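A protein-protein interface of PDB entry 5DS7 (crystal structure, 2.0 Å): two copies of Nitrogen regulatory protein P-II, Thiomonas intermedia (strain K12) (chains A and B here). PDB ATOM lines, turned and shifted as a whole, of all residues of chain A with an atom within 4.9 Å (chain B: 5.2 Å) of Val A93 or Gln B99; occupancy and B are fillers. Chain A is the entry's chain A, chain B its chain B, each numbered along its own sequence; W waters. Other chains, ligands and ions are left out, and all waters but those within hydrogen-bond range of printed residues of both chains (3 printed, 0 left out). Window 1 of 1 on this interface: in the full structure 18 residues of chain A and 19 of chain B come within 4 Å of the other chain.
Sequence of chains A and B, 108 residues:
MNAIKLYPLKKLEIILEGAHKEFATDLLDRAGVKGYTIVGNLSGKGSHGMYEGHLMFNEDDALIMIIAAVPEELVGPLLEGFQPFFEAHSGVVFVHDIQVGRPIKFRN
Val A93 touches two residues of chain B.
Printed residues of chain B within 4 Å of Lys A10: Gln B99 (3.9 Å).
Of the printed residues of chain A, Val B100 touches Val A93 (3.9 Å) and Phe A94 (3.9 Å).
Of the printed residues of chain A, Leu B6 touches Leu A79 (3.5 Å).
Of the printed residues of chain A, Ile B98 touches Phe A94 (3.8 Å) and Val A95 (3.3 Å).
Val A92 touches none of the printed residues of chain B.
The nearest printed residue of chain A that does not touch Ile B98 is Val A93 (5.9 Å).
Water W1 lies within hydrogen-bond range of the backbone carbonyl oxygen (O) of Gly A91, the guanidinium group (NH2) of Arg B102 and the backbone carbonyl oxygen (O) of Phe A86.
Water W2 lies within hydrogen-bond range of the backbone NH of Gly B101 (2.6 Å) and the backbone carbonyl oxygen of Val A93 (3.1 Å).
Water W3 bridges O of Val A95 (2.8 Å) and OE1 of Gln B99 (2.8 Å).
Of the 11 printed residues of chain A, 7 touch a printed residue of chain B.
Hydrophobic or aromatic side chains of chain B that line the printed part of chain A: Leu B6, Ile B98 and Val B100.
The backbone carbonyl oxygen of Val B100 sits at hydrogen-bond distance from the backbone NH of Tyr B7 (2.8 Å).
O of Leu B9 sits at hydrogen-bond distance from N of Ile B98, at 2.9 Å.
O of Glu A13 is in hydrogen-bond range of N of Phe A94.
NZ of Lys A10 touches OE1 of Gln B99, at 3.9 Å.
Leu A79 touches Leu B6.
Gln B99 touches Val A93.
Val A93 touches Val B100.
CD1 of Ile B98 touches CD1 of Phe A94, at 3.8 Å.
Phe A94 touches Gln B99 (C to O, 3.8 Å).
Val B100 touches Phe A94.
Val A95 touches Ile B98.
No position is printed for both chains.
Of the 11 pairs that touch across the chains among the printed residues, none has its exchanged pair printed and touching as well.
The backbone carbonyl oxygen of Phe A86 sits at hydrogen-bond distance from the guanidinium group of Arg B102 (3.0 Å).
The backbone carbonyl oxygen (O) of Gly A91 sits at hydrogen-bond distance from the guanidinium group (NH2) of Arg B102 (2.9 Å).
O of Val A95 is in hydrogen-bond range of N of Gln B99, at 2.8 Å.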
ATOM      1  N   LYS A  10     -19.230  -0.901  23.309  1.00  0.00           N
ATOM      2  CA  LYS A  10     -17.970  -1.479  22.829  1.00  0.00           C
ATOM      3  C   LYS A  10     -17.028  -0.354  22.423  1.00  0.00           C
ATOM      4  O   LYS A  10     -17.452   0.705  21.963  1.00  0.00           O
ATOM      5  CB  LYS A  10     -18.183  -2.437  21.648  1.00  0.00           C
ATOM      6  CG  LYS A  10     -19.064  -3.632  21.942  1.00  0.00           C
ATOM      7  CD  LYS A  10     -18.385  -4.650  22.830  1.00  0.00           C
ATOM      8  CE  LYS A  10     -19.331  -5.750  23.189  1.00  0.00           C
ATOM      9  NZ  LYS A  10     -18.592  -6.885  23.746  1.00  0.00           N
ATOM     10  N   LEU A  12     -13.711   0.246  20.021  1.00  0.00           N
ATOM     11  CA  LEU A  12     -12.687  -0.192  19.083  1.00  0.00           C
ATOM     12  C   LEU A  12     -11.437   0.669  19.211  1.00  0.00           C
ATOM     13  O   LEU A  12     -11.521   1.878  19.367  1.00  0.00           O
ATOM     14  CB  LEU A  12     -13.196  -0.122  17.649  1.00  0.00           C
ATOM     15  CG  LEU A  12     -14.563  -0.745  17.406  1.00  0.00           C
ATOM     16  CD1 LEU A  12     -15.068  -0.430  16.004  1.00  0.00           C
ATOM     17  CD2 LEU A  12     -14.446  -2.226  17.610  1.00  0.00           C
ATOM     18  N   GLU A  13     -10.280   0.027  19.175  1.00  0.00           N
ATOM     19  CA  GLU A  13      -9.019   0.722  18.942  1.00  0.00           C
ATOM     20  C   GLU A  13      -8.521   0.177  17.621  1.00  0.00           C
ATOM     21  O   GLU A  13      -8.266  -1.031  17.515  1.00  0.00           O
ATOM     22  CB  GLU A  13      -8.010   0.478  20.063  1.00  0.00           C
ATOM     23  CG  GLU A  13      -8.462   1.014  21.395  1.00  0.00           C
ATOM     24  CD  GLU A  13      -7.476   0.735  22.508  1.00  0.00           C
ATOM     25  OE1 GLU A  13      -7.531   1.462  23.520  1.00  0.00           O
ATOM     26  OE2 GLU A  13      -6.658  -0.202  22.380  1.00  0.00           O
ATOM     27  N   ILE A  14      -8.428   1.057  16.626  1.00  0.00           N
ATOM     28  CA  ILE A  14      -8.079   0.700  15.250  1.00  0.00           C
ATOM     29  C   ILE A  14      -6.752   1.342  14.865  1.00  0.00           C
ATOM     30  O   ILE A  14      -6.689   2.554  14.645  1.00  0.00           O
ATOM     31  CB  ILE A  14      -9.181   1.151  14.254  1.00  0.00           C
ATOM     32  CG1 ILE A  14     -10.533   0.566  14.632  1.00  0.00           C
ATOM     33  CG2 ILE A  14      -8.827   0.752  12.836  1.00  0.00           C
ATOM     34  CD1 ILE A  14     -11.713   1.423  14.178  1.00  0.00           C
ATOM     35  N   LEU A  79     -16.525  -4.552  11.499  1.00  0.00           N
ATOM     36  CA  LEU A  79     -15.402  -5.427  11.200  1.00  0.00           C
ATOM     37  C   LEU A  79     -15.480  -5.919   9.755  1.00  0.00           C
ATOM     38  O   LEU A  79     -14.462  -6.008   9.080  1.00  0.00           O
ATOM     39  CB  LEU A  79     -15.345  -6.600  12.171  1.00  0.00           C
ATOM     40  CG  LEU A  79     -15.101  -6.178  13.621  1.00  0.00           C
ATOM     41  CD1 LEU A  79     -14.837  -7.377  14.528  1.00  0.00           C
ATOM     42  CD2 LEU A  79     -13.958  -5.178  13.714  1.00  0.00           C
ATOM     43  N   PHE A  86      -7.966  -4.648   5.875  1.00  0.00           N
ATOM     44  CA  PHE A  86      -6.982  -5.261   6.769  1.00  0.00           C
ATOM     45  C   PHE A  86      -6.463  -6.604   6.246  1.00  0.00           C
ATOM     46  O   PHE A  86      -5.440  -7.070   6.708  1.00  0.00           O
ATOM     47  CB  PHE A  86      -7.553  -5.437   8.173  1.00  0.00           C
ATOM     48  CG  PHE A  86      -7.516  -4.179   8.998  1.00  0.00           C
ATOM     49  CD1 PHE A  86      -6.306  -3.555   9.275  1.00  0.00           C
ATOM     50  CD2 PHE A  86      -8.676  -3.631   9.506  1.00  0.00           C
ATOM     51  CE1 PHE A  86      -6.251  -2.404  10.036  1.00  0.00           C
ATOM     52  CE2 PHE A  86      -8.630  -2.473  10.272  1.00  0.00           C
ATOM     53  CZ  PHE A  86      -7.409  -1.857  10.533  1.00  0.00           C
ATOM     54  N   GLY A  91      -2.018  -3.427  10.220  1.00  0.00           N
ATOM     55  CA  GLY A  91      -2.877  -2.861  11.237  1.00  0.00           C
ATOM     56  C   GLY A  91      -3.680  -3.875  12.019  1.00  0.00           C
ATOM     57  O   GLY A  91      -3.810  -5.035  11.622  1.00  0.00           O
ATOM     58  N   VAL A  92      -4.221  -3.433  13.146  1.00  0.00           N
ATOM     59  CA  VAL A  92      -4.922  -4.330  14.057  1.00  0.00           C
ATOM     60  C   VAL A  92      -6.172  -3.661  14.622  1.00  0.00           C
ATOM     61  O   VAL A  92      -6.242  -2.442  14.680  1.00  0.00           O
ATOM     62  CB  VAL A  92      -4.007  -4.751  15.213  1.00  0.00           C
ATOM     63  CG1 VAL A  92      -2.842  -5.583  14.689  1.00  0.00           C
ATOM     64  CG2 VAL A  92      -3.507  -3.533  15.927  1.00  0.00           C
ATOM     65  N   VAL A  93      -7.139  -4.464  15.049  1.00  0.00           N
ATOM     66  CA  VAL A  93      -8.351  -3.962  15.692  1.00  0.00           C
ATOM     67  C   VAL A  93      -8.566  -4.658  17.039  1.00  0.00           C
ATOM     68  O   VAL A  93      -8.613  -5.877  17.115  1.00  0.00           O
ATOM     69  CB  VAL A  93      -9.587  -4.173  14.805  1.00  0.00           C
ATOM     70  CG1 VAL A  93     -10.836  -3.746  15.539  1.00  0.00           C
ATOM     71  CG2 VAL A  93      -9.438  -3.410  13.513  1.00  0.00           C
ATOM     72  N   PHE A  94      -8.667  -3.877  18.111  1.00  0.00           N
ATOM     73  CA  PHE A  94      -8.918  -4.423  19.448  1.00  0.00           C
ATOM     74  C   PHE A  94     -10.326  -4.034  19.923  1.00  0.00           C
ATOM     75  O   PHE A  94     -10.669  -2.851  19.930  1.00  0.00           O
ATOM     76  CB  PHE A  94      -7.877  -3.909  20.446  1.00  0.00           C
ATOM     77  CG  PHE A  94      -6.438  -4.163  20.042  1.00  0.00           C
ATOM     78  CD1 PHE A  94      -6.091  -5.257  19.272  1.00  0.00           C
ATOM     79  CD2 PHE A  94      -5.431  -3.295  20.458  1.00  0.00           C
ATOM     80  CE1 PHE A  94      -4.779  -5.481  18.927  1.00  0.00           C
ATOM     81  CE2 PHE A  94      -4.116  -3.521  20.115  1.00  0.00           C
ATOM     82  CZ  PHE A  94      -3.792  -4.602  19.341  1.00  0.00           C
ATOM     83  N   VAL A  95     -11.138  -5.013  20.310  1.00  0.00           N
ATOM     84  CA  VAL A  95     -12.491  -4.734  20.794  1.00  0.00           C
ATOM     85  C   VAL A  95     -12.530  -4.792  22.325  1.00  0.00           C
ATOM     86  O   VAL A  95     -12.201  -5.828  22.901  1.00  0.00           O
ATOM     87  CB  VAL A  95     -13.528  -5.741  20.210  1.00  0.00           C
ATOM     88  CG1 VAL A  95     -14.936  -5.381  20.654  1.00  0.00           C
ATOM     89  CG2 VAL A  95     -13.444  -5.772  18.706  1.00  0.00           C
ATOM     90  N   LEU B   6     -14.840 -13.544  16.798  1.00  0.00           N
ATOM     91  CA  LEU B   6     -13.980 -12.811  17.724  1.00  0.00           C
ATOM     92  C   LEU B   6     -13.414 -13.735  18.792  1.00  0.00           C
ATOM     93  O   LEU B   6     -14.110 -14.603  19.307  1.00  0.00           O
ATOM     94  CB  LEU B   6     -14.753 -11.660  18.376  1.00  0.00           C
ATOM     95  CG  LEU B   6     -15.184 -10.524  17.447  1.00  0.00           C
ATOM     96  CD1 LEU B   6     -15.936  -9.481  18.233  1.00  0.00           C
ATOM     97  CD2 LEU B   6     -13.988  -9.886  16.760  1.00  0.00           C
ATOM     98  N   TYR B   7     -12.145 -13.544  19.122  1.00  0.00           N
ATOM     99  CA  TYR B   7     -11.462 -14.402  20.072  1.00  0.00           C
ATOM    100  C   TYR B   7     -10.911 -13.554  21.210  1.00  0.00           C
ATOM    101  O   TYR B   7     -10.578 -12.384  20.987  1.00  0.00           O
ATOM    102  CB  TYR B   7     -10.337 -15.162  19.373  1.00  0.00           C
ATOM    103  CG  TYR B   7     -10.760 -15.950  18.143  1.00  0.00           C
ATOM    104  CD1 TYR B   7     -10.950 -15.325  16.910  1.00  0.00           C
ATOM    105  CD2 TYR B   7     -10.938 -17.327  18.211  1.00  0.00           C
ATOM    106  CE1 TYR B   7     -11.323 -16.052  15.778  1.00  0.00           C
ATOM    107  CE2 TYR B   7     -11.311 -18.062  17.092  1.00  0.00           C
ATOM    108  CZ  TYR B   7     -11.500 -17.425  15.883  1.00  0.00           C
ATOM    109  OH  TYR B   7     -11.864 -18.163  14.783  1.00  0.00           O
ATOM    110  N   PRO B   8     -10.836 -14.115  22.435  1.00  0.00           N
ATOM    111  CA  PRO B   8     -10.312 -13.349  23.570  1.00  0.00           C
ATOM    112  C   PRO B   8      -8.802 -13.220  23.528  1.00  0.00           C
ATOM    113  O   PRO B   8      -8.122 -14.101  23.039  1.00  0.00           O
ATOM    114  CB  PRO B   8     -10.744 -14.175  24.783  1.00  0.00           C
ATOM    115  CG  PRO B   8     -10.871 -15.534  24.262  1.00  0.00           C
ATOM    116  CD  PRO B   8     -11.361 -15.420  22.868  1.00  0.00           C
ATOM    117  N   LEU B   9      -8.158 -12.195  23.958  1.00  0.00           N
ATOM    118  CA  LEU B   9      -6.789 -11.949  24.372  1.00  0.00           C
ATOM    119  C   LEU B   9      -6.869 -10.950  25.516  1.00  0.00           C
ATOM    120  O   LEU B   9      -7.961 -10.458  25.849  1.00  0.00           O
ATOM    121  CB  LEU B   9      -5.932 -11.376  23.244  1.00  0.00           C
ATOM    122  CG  LEU B   9      -5.560 -12.094  21.949  1.00  0.00           C
ATOM    123  CD1 LEU B   9      -4.814 -11.100  21.030  1.00  0.00           C
ATOM    124  CD2 LEU B   9      -4.729 -13.344  22.184  1.00  0.00           C
ATOM    125  N   ASP B  97      -8.997  -7.120  29.192  1.00  0.00           N
ATOM    126  CA  ASP B  97      -9.582  -8.136  28.326  1.00  0.00           C
ATOM    127  C   ASP B  97      -9.941  -7.484  27.007  1.00  0.00           C
ATOM    128  O   ASP B  97     -10.554  -6.420  27.010  1.00  0.00           O
ATOM    129  CB  ASP B  97     -10.856  -8.738  28.921  1.00  0.00           C
ATOM    130  CG  ASP B  97     -10.592  -9.675  30.059  1.00  0.00           C
ATOM    131  OD1 ASP B  97      -9.543 -10.343  30.058  1.00  0.00           O
ATOM    132  OD2 ASP B  97     -11.448  -9.745  30.964  1.00  0.00           O
ATOM    133  N   ILE B  98      -9.572  -8.091  25.884  1.00  0.00           N
ATOM    134  CA  ILE B  98     -10.051  -7.589  24.591  1.00  0.00           C
ATOM    135  C   ILE B  98     -10.502  -8.739  23.709  1.00  0.00           C
ATOM    136  O   ILE B  98     -10.344  -9.903  24.066  1.00  0.00           O
ATOM    137  CB  ILE B  98      -8.977  -6.794  23.819  1.00  0.00           C
ATOM    138  CG1 ILE B  98      -7.737  -7.647  23.578  1.00  0.00           C
ATOM    139  CG2 ILE B  98      -8.596  -5.525  24.549  1.00  0.00           C
ATOM    140  CD1 ILE B  98      -6.806  -7.027  22.579  1.00  0.00           C
ATOM    141  N   GLN B  99     -11.065  -8.404  22.556  1.00  0.00           N
ATOM    142  CA  GLN B  99     -11.337  -9.405  21.535  1.00  0.00           C
ATOM    143  C   GLN B  99     -10.672  -8.982  20.242  1.00  0.00           C
ATOM    144  O   GLN B  99     -10.534  -7.782  19.961  1.00  0.00           O
ATOM    145  CB  GLN B  99     -12.838  -9.588  21.315  1.00  0.00           C
ATOM    146  CG  GLN B  99     -13.614 -10.053  22.537  1.00  0.00           C
ATOM    147  CD  GLN B  99     -15.103 -10.093  22.259  1.00  0.00           C
ATOM    148  OE1 GLN B  99     -15.765  -9.052  22.186  1.00  0.00           O
ATOM    149  NE2 GLN B  99     -15.636 -11.298  22.082  1.00  0.00           N
ATOM    150  N   VAL B 100     -10.259  -9.971  19.457  1.00  0.00           N
ATOM    151  CA  VAL B 100      -9.668  -9.729  18.157  1.00  0.00           C
ATOM    152  C   VAL B 100     -10.217 -10.733  17.148  1.00  0.00           C
ATOM    153  O   VAL B 100     -10.695 -11.796  17.519  1.00  0.00           O
ATOM    154  CB  VAL B 100      -8.139  -9.840  18.188  1.00  0.00           C
ATOM    155  CG1 VAL B 100      -7.557  -8.906  19.248  1.00  0.00           C
ATOM    156  CG2 VAL B 100      -7.707 -11.301  18.469  1.00  0.00           C
ATOM    157  N   GLY B 101     -10.127 -10.391  15.870  1.00  0.00           N
ATOM    158  CA  GLY B 101     -10.604 -11.278  14.823  1.00  0.00           C
ATOM    159  C   GLY B 101      -9.546 -12.203  14.245  1.00  0.00           C
ATOM    160  O   GLY B 101      -9.885 -13.119  13.515  1.00  0.00           O
ATOM    161  N   ARG B 102      -8.272 -11.988  14.573  1.00  0.00           N
ATOM    162  CA  ARG B 102      -7.195 -12.791  13.979  1.00  0.00           C
ATOM    163  C   ARG B 102      -6.139 -13.226  14.998  1.00  0.00           C
ATOM    164  O   ARG B 102      -5.067 -12.616  15.089  1.00  0.00           O
ATOM    165  CB  ARG B 102      -6.526 -12.000  12.857  1.00  0.00           C
ATOM    166  CG  ARG B 102      -7.491 -11.592  11.757  1.00  0.00           C
ATOM    167  CD  ARG B 102      -6.836 -10.691  10.744  1.00  0.00           C
ATOM    168  NE  ARG B 102      -6.519  -9.384  11.308  1.00  0.00           N
ATOM    169  CZ  ARG B 102      -5.981  -8.390  10.617  1.00  0.00           C
ATOM    170  NH1 ARG B 102      -5.702  -8.550   9.325  1.00  0.00           N
ATOM    171  NH2 ARG B 102      -5.716  -7.240  11.220  1.00  0.00           N
HETATM  172  O   HOH W   1      -3.561  -6.069   9.247  1.00  0.00           O
HETATM  173  O   HOH W   2      -8.771  -8.247  15.110  1.00  0.00           O
HETATM  174  O   HOH W   3     -14.698  -6.818  23.594  1.00  0.00           O
